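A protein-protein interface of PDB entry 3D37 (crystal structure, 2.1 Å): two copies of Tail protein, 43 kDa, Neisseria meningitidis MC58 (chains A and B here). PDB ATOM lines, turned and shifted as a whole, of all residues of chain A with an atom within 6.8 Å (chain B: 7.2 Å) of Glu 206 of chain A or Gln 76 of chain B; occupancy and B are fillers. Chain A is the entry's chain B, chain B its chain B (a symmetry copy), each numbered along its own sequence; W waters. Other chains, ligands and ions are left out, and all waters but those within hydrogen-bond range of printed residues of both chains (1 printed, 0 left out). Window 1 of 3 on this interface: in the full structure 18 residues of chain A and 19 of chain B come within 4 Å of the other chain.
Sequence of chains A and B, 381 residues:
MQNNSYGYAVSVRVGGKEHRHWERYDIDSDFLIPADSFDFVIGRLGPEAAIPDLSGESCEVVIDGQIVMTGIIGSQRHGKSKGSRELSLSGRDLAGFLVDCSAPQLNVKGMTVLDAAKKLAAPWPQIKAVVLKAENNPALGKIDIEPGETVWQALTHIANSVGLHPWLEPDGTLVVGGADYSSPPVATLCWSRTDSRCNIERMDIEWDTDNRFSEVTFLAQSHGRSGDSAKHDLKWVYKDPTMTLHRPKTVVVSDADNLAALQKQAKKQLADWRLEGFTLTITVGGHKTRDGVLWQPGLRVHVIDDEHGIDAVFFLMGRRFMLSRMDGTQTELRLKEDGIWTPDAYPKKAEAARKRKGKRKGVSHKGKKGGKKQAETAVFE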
ATOM      1  N   ASP A 204     -17.241 -25.424 -17.974  1.00  0.00           N
ATOM      2  CA  ASP A 204     -16.865 -24.386 -18.946  1.00  0.00           C
ATOM      3  C   ASP A 204     -15.792 -23.523 -18.363  1.00  0.00           C
ATOM      4  O   ASP A 204     -15.961 -22.971 -17.293  1.00  0.00           O
ATOM      5  CB  ASP A 204     -18.061 -23.502 -19.268  1.00  0.00           C
ATOM      6  CG  ASP A 204     -19.124 -24.234 -20.022  1.00  0.00           C
ATOM      7  OD1 ASP A 204     -18.879 -24.575 -21.175  1.00  0.00           O
ATOM      8  OD2 ASP A 204     -20.209 -24.487 -19.454  1.00  0.00           O
ATOM      9  N   ILE A 205     -14.668 -23.446 -19.053  1.00  0.00           N
ATOM     10  CA  ILE A 205     -13.563 -22.661 -18.599  1.00  0.00           C
ATOM     11  C   ILE A 205     -13.333 -21.518 -19.620  1.00  0.00           C
ATOM     12  O   ILE A 205     -13.258 -21.761 -20.821  1.00  0.00           O
ATOM     13  CB  ILE A 205     -12.260 -23.454 -18.439  1.00  0.00           C
ATOM     14  CG1 ILE A 205     -12.471 -24.719 -17.596  1.00  0.00           C
ATOM     15  CG2 ILE A 205     -11.208 -22.516 -17.824  1.00  0.00           C
ATOM     16  CD1 ILE A 205     -11.201 -25.551 -17.403  1.00  0.00           C
ATOM     17  N   GLU A 206     -13.240 -20.289 -19.111  1.00  0.00           N
ATOM     18  CA  GLU A 206     -13.006 -19.095 -19.943  1.00  0.00           C
ATOM     19  C   GLU A 206     -11.814 -18.296 -19.450  1.00  0.00           C
ATOM     20  O   GLU A 206     -11.682 -17.963 -18.272  1.00  0.00           O
ATOM     21  CB  GLU A 206     -14.259 -18.210 -19.988  1.00  0.00           C
ATOM     22  CG  GLU A 206     -15.516 -19.039 -20.274  1.00  0.00           C
ATOM     23  CD  GLU A 206     -16.828 -18.251 -20.397  1.00  0.00           C
ATOM     24  OE1 GLU A 206     -17.265 -17.621 -19.382  1.00  0.00           O
ATOM     25  OE2 GLU A 206     -17.433 -18.303 -21.507  1.00  0.00           O
ATOM     26  N   TRP A 207     -10.931 -18.017 -20.386  1.00  0.00           N
ATOM     27  CA  TRP A 207      -9.808 -17.140 -20.207  1.00  0.00           C
ATOM     28  C   TRP A 207     -10.009 -15.993 -21.206  1.00  0.00           C
ATOM     29  O   TRP A 207     -10.323 -16.206 -22.348  1.00  0.00           O
ATOM     30  CB  TRP A 207      -8.486 -17.823 -20.522  1.00  0.00           C
ATOM     31  CG  TRP A 207      -8.116 -19.039 -19.729  1.00  0.00           C
ATOM     32  CD1 TRP A 207      -7.332 -19.092 -18.600  1.00  0.00           C
ATOM     33  CD2 TRP A 207      -8.451 -20.395 -20.047  1.00  0.00           C
ATOM     34  NE1 TRP A 207      -7.189 -20.406 -18.183  1.00  0.00           N
ATOM     35  CE2 TRP A 207      -7.847 -21.224 -19.066  1.00  0.00           C
ATOM     36  CE3 TRP A 207      -9.212 -20.995 -21.067  1.00  0.00           C
ATOM     37  CZ2 TRP A 207      -7.999 -22.623 -19.067  1.00  0.00           C
ATOM     38  CZ3 TRP A 207      -9.361 -22.392 -21.077  1.00  0.00           C
ATOM     39  CH2 TRP A 207      -8.759 -23.187 -20.067  1.00  0.00           C
ATOM     40  N   ASP A 208      -9.805 -14.774 -20.733  1.00  0.00           N
ATOM     41  CA  ASP A 208     -10.035 -13.569 -21.504  1.00  0.00           C
ATOM     42  C   ASP A 208      -8.883 -12.615 -21.145  1.00  0.00           C
ATOM     43  O   ASP A 208      -8.531 -12.452 -19.960  1.00  0.00           O
ATOM     44  CB  ASP A 208     -11.391 -12.978 -21.099  1.00  0.00           C
ATOM     45  CG  ASP A 208     -11.646 -11.603 -21.704  1.00  0.00           C
ATOM     46  OD1 ASP A 208     -10.803 -11.079 -22.478  1.00  0.00           O
ATOM     47  OD2 ASP A 208     -12.708 -11.019 -21.393  1.00  0.00           O
ATOM     48  N   THR A 209      -8.291 -12.017 -22.166  1.00  0.00           N
ATOM     49  CA  THR A 209      -7.197 -11.076 -21.963  1.00  0.00           C
ATOM     50  C   THR A 209      -7.584  -9.611 -22.073  1.00  0.00           C
ATOM     51  O   THR A 209      -6.712  -8.779 -21.970  1.00  0.00           O
ATOM     52  CB  THR A 209      -6.055 -11.312 -22.970  1.00  0.00           C
ATOM     53  OG1 THR A 209      -6.503 -10.951 -24.291  1.00  0.00           O
ATOM     54  CG2 THR A 209      -5.605 -12.726 -22.939  1.00  0.00           C
ATOM     55  N   GLU A 276     -11.739 -10.823 -13.795  1.00  0.00           N
ATOM     56  CA  GLU A 276     -12.464 -10.855 -15.069  1.00  0.00           C
ATOM     57  C   GLU A 276     -11.821 -11.772 -16.083  1.00  0.00           C
ATOM     58  O   GLU A 276     -12.477 -12.212 -16.975  1.00  0.00           O
ATOM     59  CB  GLU A 276     -12.581  -9.488 -15.727  1.00  0.00           C
ATOM     60  CG  GLU A 276     -13.387  -8.461 -14.966  1.00  0.00           C
ATOM     61  CD  GLU A 276     -13.250  -7.079 -15.583  1.00  0.00           C
ATOM     62  OE1 GLU A 276     -12.821  -7.007 -16.738  1.00  0.00           O
ATOM     63  OE2 GLU A 276     -13.565  -6.076 -14.921  1.00  0.00           O
ATOM     64  N   GLY A 277     -10.532 -12.036 -15.941  1.00  0.00           N
ATOM     65  CA  GLY A 277      -9.757 -12.787 -16.912  1.00  0.00           C
ATOM     66  C   GLY A 277      -9.935 -14.288 -16.860  1.00  0.00           C
ATOM     67  O   GLY A 277      -9.533 -14.968 -17.796  1.00  0.00           O
ATOM     68  N   PHE A 278     -10.596 -14.809 -15.820  1.00  0.00           N
ATOM     69  CA  PHE A 278     -10.796 -16.243 -15.715  1.00  0.00           C
ATOM     70  C   PHE A 278     -12.096 -16.578 -15.012  1.00  0.00           C
ATOM     71  O   PHE A 278     -12.415 -16.044 -13.941  1.00  0.00           O
ATOM     72  CB  PHE A 278      -9.600 -16.881 -14.986  1.00  0.00           C
ATOM     73  CG  PHE A 278      -9.798 -18.319 -14.632  1.00  0.00           C
ATOM     74  CD1 PHE A 278      -9.484 -19.327 -15.543  1.00  0.00           C
ATOM     75  CD2 PHE A 278     -10.280 -18.675 -13.378  1.00  0.00           C
ATOM     76  CE1 PHE A 278      -9.629 -20.660 -15.215  1.00  0.00           C
ATOM     77  CE2 PHE A 278     -10.438 -20.028 -13.036  1.00  0.00           C
ATOM     78  CZ  PHE A 278     -10.114 -21.014 -13.946  1.00  0.00           C
ATOM     79  N   THR A 279     -12.857 -17.441 -15.627  1.00  0.00           N
ATOM     80  CA  THR A 279     -14.065 -17.997 -15.022  1.00  0.00           C
ATOM     81  C   THR A 279     -14.153 -19.503 -15.286  1.00  0.00           C
ATOM     82  O   THR A 279     -13.968 -19.974 -16.419  1.00  0.00           O
ATOM     83  CB  THR A 279     -15.366 -17.310 -15.506  1.00  0.00           C
ATOM     84  OG1 THR A 279     -15.205 -15.873 -15.455  1.00  0.00           O
ATOM     85  CG2 THR A 279     -16.535 -17.688 -14.571  1.00  0.00           C
ATOM     86  N   LEU A 280     -14.447 -20.226 -14.203  1.00  0.00           N
ATOM     87  CA  LEU A 280     -14.748 -21.644 -14.192  1.00  0.00           C
ATOM     88  C   LEU A 280     -16.222 -21.825 -13.854  1.00  0.00           C
ATOM     89  O   LEU A 280     -16.662 -21.579 -12.726  1.00  0.00           O
ATOM     90  CB  LEU A 280     -13.894 -22.342 -13.140  1.00  0.00           C
ATOM     91  CG  LEU A 280     -14.145 -23.835 -12.911  1.00  0.00           C
ATOM     92  CD1 LEU A 280     -13.918 -24.609 -14.176  1.00  0.00           C
ATOM     93  CD2 LEU A 280     -13.211 -24.278 -11.888  1.00  0.00           C
ATOM     94  N   THR A 281     -16.977 -22.235 -14.838  1.00  0.00           N
ATOM     95  CA  THR A 281     -18.399 -22.475 -14.666  1.00  0.00           C
ATOM     96  C   THR A 281     -18.674 -24.001 -14.639  1.00  0.00           C
ATOM     97  O   THR A 281     -18.484 -24.703 -15.649  1.00  0.00           O
ATOM     98  CB  THR A 281     -19.238 -21.777 -15.760  1.00  0.00           C
ATOM     99  OG1 THR A 281     -18.745 -20.430 -15.950  1.00  0.00           O
ATOM    100  CG2 THR A 281     -20.709 -21.755 -15.396  1.00  0.00           C
ATOM    101  N   LYS A 336     -14.313 -18.548  -9.261  1.00  0.00           N
ATOM    102  CA  LYS A 336     -13.166 -17.688  -9.579  1.00  0.00           C
ATOM    103  C   LYS A 336     -11.888 -18.152  -8.895  1.00  0.00           C
ATOM    104  O   LYS A 336     -11.940 -18.921  -7.941  1.00  0.00           O
ATOM    105  CB  LYS A 336     -13.484 -16.243  -9.137  1.00  0.00           C
ATOM    106  CG  LYS A 336     -14.606 -15.591  -9.939  1.00  0.00           C
ATOM    107  CD  LYS A 336     -14.124 -15.320 -11.392  1.00  0.00           C
ATOM    108  CE  LYS A 336     -14.988 -14.370 -12.150  1.00  0.00           C
ATOM    109  NZ  LYS A 336     -14.459 -14.104 -13.519  1.00  0.00           N
ATOM    110  N   PRO B  52      -4.125 -26.133 -22.408  1.00  0.00           N
ATOM    111  CA  PRO B  52      -3.047 -25.138 -22.458  1.00  0.00           C
ATOM    112  C   PRO B  52      -3.584 -23.685 -22.720  1.00  0.00           C
ATOM    113  O   PRO B  52      -4.271 -23.467 -23.719  1.00  0.00           O
ATOM    114  CB  PRO B  52      -2.207 -25.631 -23.642  1.00  0.00           C
ATOM    115  CG  PRO B  52      -3.272 -26.270 -24.598  1.00  0.00           C
ATOM    116  CD  PRO B  52      -4.513 -26.569 -23.762  1.00  0.00           C
ATOM    117  N   ASP B  53      -3.287 -22.727 -21.843  1.00  0.00           N
ATOM    118  CA  ASP B  53      -3.853 -21.385 -21.994  1.00  0.00           C
ATOM    119  C   ASP B  53      -3.122 -20.529 -23.033  1.00  0.00           C
ATOM    120  O   ASP B  53      -2.098 -19.931 -22.717  1.00  0.00           O
ATOM    121  CB  ASP B  53      -3.879 -20.635 -20.661  1.00  0.00           C
ATOM    122  CG  ASP B  53      -4.442 -19.221 -20.791  1.00  0.00           C
ATOM    123  OD1 ASP B  53      -5.291 -18.972 -21.683  1.00  0.00           O
ATOM    124  OD2 ASP B  53      -4.046 -18.351 -19.991  1.00  0.00           O
ATOM    125  N   LEU B  54      -3.704 -20.426 -24.231  1.00  0.00           N
ATOM    126  CA  LEU B  54      -3.150 -19.633 -25.342  1.00  0.00           C
ATOM    127  C   LEU B  54      -3.602 -18.152 -25.389  1.00  0.00           C
ATOM    128  O   LEU B  54      -3.197 -17.411 -26.294  1.00  0.00           O
ATOM    129  CB  LEU B  54      -3.530 -20.298 -26.679  1.00  0.00           C
ATOM    130  CG  LEU B  54      -3.185 -21.785 -26.816  1.00  0.00           C
ATOM    131  CD1 LEU B  54      -3.524 -22.276 -28.198  1.00  0.00           C
ATOM    132  CD2 LEU B  54      -1.730 -22.015 -26.489  1.00  0.00           C
ATOM    133  N   SER B  55      -4.436 -17.714 -24.442  1.00  0.00           N
ATOM    134  CA  SER B  55      -5.029 -16.378 -24.553  1.00  0.00           C
ATOM    135  C   SER B  55      -3.957 -15.330 -24.292  1.00  0.00           C
ATOM    136  O   SER B  55      -3.125 -15.483 -23.401  1.00  0.00           O
ATOM    137  CB  SER B  55      -6.257 -16.204 -23.643  1.00  0.00           C
ATOM    138  OG  SER B  55      -5.920 -16.119 -22.278  1.00  0.00           O
ATOM    139  N   GLY B  56      -3.960 -14.283 -25.106  1.00  0.00           N
ATOM    140  CA  GLY B  56      -2.918 -13.277 -25.064  1.00  0.00           C
ATOM    141  C   GLY B  56      -1.751 -13.564 -25.980  1.00  0.00           C
ATOM    142  O   GLY B  56      -0.932 -12.672 -26.184  1.00  0.00           O
ATOM    143  N   ILE B  73      -4.647 -13.945 -29.927  1.00  0.00           N
ATOM    144  CA  ILE B  73      -5.741 -14.681 -29.300  1.00  0.00           C
ATOM    145  C   ILE B  73      -6.285 -13.858 -28.133  1.00  0.00           C
ATOM    146  O   ILE B  73      -5.582 -13.612 -27.184  1.00  0.00           O
ATOM    147  CB  ILE B  73      -5.204 -16.029 -28.805  1.00  0.00           C
ATOM    148  CG1 ILE B  73      -4.856 -16.881 -30.036  1.00  0.00           C
ATOM    149  CG2 ILE B  73      -6.270 -16.792 -27.936  1.00  0.00           C
ATOM    150  CD1 ILE B  73      -4.162 -18.065 -29.741  1.00  0.00           C
ATOM    151  N   GLY B  74      -7.517 -13.386 -28.222  1.00  0.00           N
ATOM    152  CA  GLY B  74      -8.122 -12.594 -27.165  1.00  0.00           C
ATOM    153  C   GLY B  74      -8.746 -13.416 -26.060  1.00  0.00           C
ATOM    154  O   GLY B  74      -8.803 -12.997 -24.930  1.00  0.00           O
ATOM    155  N   SER B  75      -9.268 -14.566 -26.412  1.00  0.00           N
ATOM    156  CA  SER B  75     -10.056 -15.376 -25.501  1.00  0.00           C
ATOM    157  C   SER B  75     -10.044 -16.850 -25.925  1.00  0.00           C
ATOM    158  O   SER B  75      -9.879 -17.220 -27.107  1.00  0.00           O
ATOM    159  CB  SER B  75     -11.494 -14.857 -25.436  1.00  0.00           C
ATOM    160  OG  SER B  75     -12.147 -15.291 -26.576  1.00  0.00           O
ATOM    161  N   GLN B  76     -10.132 -17.690 -24.909  1.00  0.00           N
ATOM    162  CA  GLN B  76     -10.118 -19.121 -25.079  1.00  0.00           C
ATOM    163  C   GLN B  76     -11.211 -19.684 -24.229  1.00  0.00           C
ATOM    164  O   GLN B  76     -11.452 -19.208 -23.125  1.00  0.00           O
ATOM    165  CB  GLN B  76      -8.776 -19.678 -24.615  1.00  0.00           C
ATOM    166  CG  GLN B  76      -8.617 -21.198 -24.723  1.00  0.00           C
ATOM    167  CD  GLN B  76      -7.160 -21.668 -24.496  1.00  0.00           C
ATOM    168  OE1 GLN B  76      -6.221 -20.899 -24.602  1.00  0.00           O
ATOM    169  NE2 GLN B  76      -6.997 -22.931 -24.175  1.00  0.00           N
ATOM    170  N   ARG B  77     -11.857 -20.723 -24.729  1.00  0.00           N
ATOM    171  CA  ARG B  77     -12.863 -21.421 -23.946  1.00  0.00           C
ATOM    172  C   ARG B  77     -12.664 -22.930 -24.064  1.00  0.00           C
ATOM    173  O   ARG B  77     -12.462 -23.457 -25.134  1.00  0.00           O
ATOM    174  CB  ARG B  77     -14.288 -21.011 -24.364  1.00  0.00           C
ATOM    175  CG  ARG B  77     -15.302 -21.338 -23.256  1.00  0.00           C
ATOM    176  CD  ARG B  77     -16.724 -21.527 -23.736  1.00  0.00           C
ATOM    177  NE  ARG B  77     -16.859 -22.863 -24.316  1.00  0.00           N
ATOM    178  CZ  ARG B  77     -17.877 -23.694 -24.121  1.00  0.00           C
ATOM    179  NH1 ARG B  77     -17.862 -24.862 -24.739  1.00  0.00           N
ATOM    180  NH2 ARG B  77     -18.904 -23.377 -23.331  1.00  0.00           N
ATOM    181  N   HIS B  78     -12.678 -23.603 -22.926  1.00  0.00           N
ATOM    182  CA  HIS B  78     -12.746 -25.038 -22.915  1.00  0.00           C
ATOM    183  C   HIS B  78     -14.074 -25.493 -22.301  1.00  0.00           C
ATOM    184  O   HIS B  78     -14.329 -25.246 -21.115  1.00  0.00           O
ATOM    185  CB  HIS B  78     -11.578 -25.693 -22.170  1.00  0.00           C
ATOM    186  CG  HIS B  78     -11.648 -27.190 -22.252  1.00  0.00           C
ATOM    187  ND1 HIS B  78     -11.702 -27.860 -23.459  1.00  0.00           N
ATOM    188  CD2 HIS B  78     -11.801 -28.131 -21.297  1.00  0.00           C
ATOM    189  CE1 HIS B  78     -11.852 -29.150 -23.238  1.00  0.00           C
ATOM    190  NE2 HIS B  78     -11.900 -29.341 -21.932  1.00  0.00           N
ATOM    191  N   LEU B  87     -12.785 -26.901 -27.506  1.00  0.00           N
ATOM    192  CA  LEU B  87     -11.809 -25.912 -27.199  1.00  0.00           C
ATOM    193  C   LEU B  87     -11.996 -24.871 -28.264  1.00  0.00           C
ATOM    194  O   LEU B  87     -11.982 -25.191 -29.444  1.00  0.00           O
ATOM    195  CB  LEU B  87     -10.406 -26.506 -27.266  1.00  0.00           C
ATOM    196  CG  LEU B  87      -9.225 -25.546 -27.007  1.00  0.00           C
ATOM    197  CD1 LEU B  87      -9.245 -24.828 -25.604  1.00  0.00           C
ATOM    198  CD2 LEU B  87      -7.884 -26.320 -27.231  1.00  0.00           C
ATOM    199  N   SER B  88     -12.242 -23.627 -27.856  1.00  0.00           N
ATOM    200  CA  SER B  88     -12.336 -22.556 -28.849  1.00  0.00           C
ATOM    201  C   SER B  88     -11.326 -21.455 -28.528  1.00  0.00           C
ATOM    202  O   SER B  88     -10.960 -21.261 -27.384  1.00  0.00           O
ATOM    203  CB  SER B  88     -13.753 -22.003 -28.992  1.00  0.00           C
ATOM    204  OG  SER B  88     -14.211 -21.583 -27.735  1.00  0.00           O
ATOM    205  N   LEU B  89     -10.876 -20.812 -29.604  1.00  0.00           N
ATOM    206  CA  LEU B  89      -9.964 -19.668 -29.606  1.00  0.00           C
ATOM    207  C   LEU B  89     -10.555 -18.592 -30.498  1.00  0.00           C
ATOM    208  O   LEU B  89     -11.012 -18.866 -31.634  1.00  0.00           O
ATOM    209  CB  LEU B  89      -8.610 -20.066 -30.207  1.00  0.00           C
ATOM    210  CG  LEU B  89      -7.899 -21.260 -29.575  1.00  0.00           C
ATOM    211  CD1 LEU B  89      -6.772 -21.733 -30.454  1.00  0.00           C
ATOM    212  CD2 LEU B  89      -7.402 -20.905 -28.181  1.00  0.00           C
ATOM    213  N   SER B  90     -10.542 -17.353 -30.013  1.00  0.00           N
ATOM    214  CA  SER B  90     -10.864 -16.256 -30.881  1.00  0.00           C
ATOM    215  C   SER B  90      -9.938 -15.075 -30.674  1.00  0.00           C
ATOM    216  O   SER B  90      -9.261 -14.994 -29.678  1.00  0.00           O
ATOM    217  CB  SER B  90     -12.332 -15.862 -30.711  1.00  0.00           C
ATOM    218  OG  SER B  90     -12.646 -15.705 -29.365  1.00  0.00           O
HETATM  219  O   HOH W   1     -11.493 -10.992 -25.333  1.00  0.00           O
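O of Trp 207 of chain A sits at hydrogen-bond distance from N of Gln 76 of chain B.
N of Thr 209 of chain A lies within hydrogen-bond range of O of Gly 74 of chain B (3.0 Å).
OD1 of Asp 204 of chain A lies within salt-bridge range of NH2 of Arg 77 of chain B, 2.5 Å away.
The backbone carbonyl oxygen (O) of His 78 of chain B lies within hydrogen-bond range of the backbone NH (N) of Ile 205 of chain A, 2.8 Å away.
The backbone NH (N) of Gly 56 of chain B lies within hydrogen-bond range of the backbone carbonyl oxygen (O) of Ile 73 of chain B, 2.7 Å away.
N of Asp 204 of chain A lies within hydrogen-bond range of O of Thr 281 of chain A.
The side-chain hydroxyl (OG) of Ser 90 of chain B lies within hydrogen-bond range of the side-chain hydroxyl (OG) of Ser 75 of chain B (2.9 Å).
N of Glu 206 of chain A sits at hydrogen-bond distance from O of Thr 279 of chain A (2.8 Å).
OE1 of Gln 76 of chain B sits at hydrogen-bond distance from N of Leu 54 of chain B (2.6 Å).
N of Gly 74 of chain B lies within hydrogen-bond range of O of Ser 90 of chain B, 2.8 Å away.
CA of Asp 204 of chain A touches O of His 78 of chain B (3.4 Å).
Ile 205 of chain A touches Gln 76 of chain B (O to O, 3.9 Å).
Arg 77 of chain B touches Ile 205 of chain A.
Arg 77 of chain B touches Glu 206 of chain A.
Trp 207 of chain A touches Asp 53 of chain B.
CB of Trp 207 of chain A touches OG of Ser 55 of chain B, at 3.5 Å.
Ser 75 of chain B touches Trp 207 of chain A (CA to O, 3.3 Å).
CZ3 of Trp 207 of chain A touches N of His 78 of chain B, at 3.99 Å.
CG2 of Thr 209 of chain A touches C of Ser 55 of chain B, at 3.4 Å.
N of Gly 56 of chain B touches CG2 of Thr 209 of chain A, at 3.1 Å.
Glu 206 of chain A touches two residues of chain B.
Thr 281 of chain A touches none of the printed residues of chain B.
Of the printed residues of chain A, Gly 74 of chain B touches Asp 208 (3.7 Å) and Thr 209 (3.0 Å).
Gln 76 of chain B touches just these residues of chain A: Ile 205 (3.9 Å), Glu 206 (3.5 Å) and Trp 207 (3.0 Å).
Of the printed residues of chain A, Arg 77 of chain B touches Asp 204, Ile 205 and Glu 206.
Leu 87 of chain B touches none of the printed residues of chain A.
The nearest printed residue of chain A that does not touch Arg 77 of chain B is Trp 207 of chain A (4.5 Å).
Of the 13 printed residues of chain A, 6 touch a printed residue of chain B.
Of the 15 printed residues of chain B, 8 touch a printed residue of chain A.
Along chain B the printed residues that touch a printed residue of chain A span positions 53 to 78.
Among the printed residues, 16 pairs touch across the chains.
No position is printed for both chains.
Water W1 lies within hydrogen-bond range of the side-chain carboxylate (OD1) of Asp 208 of chain A (2.9 Å) and the backbone carbonyl oxygen (O) of Gly 74 of chain B (3.4 Å).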
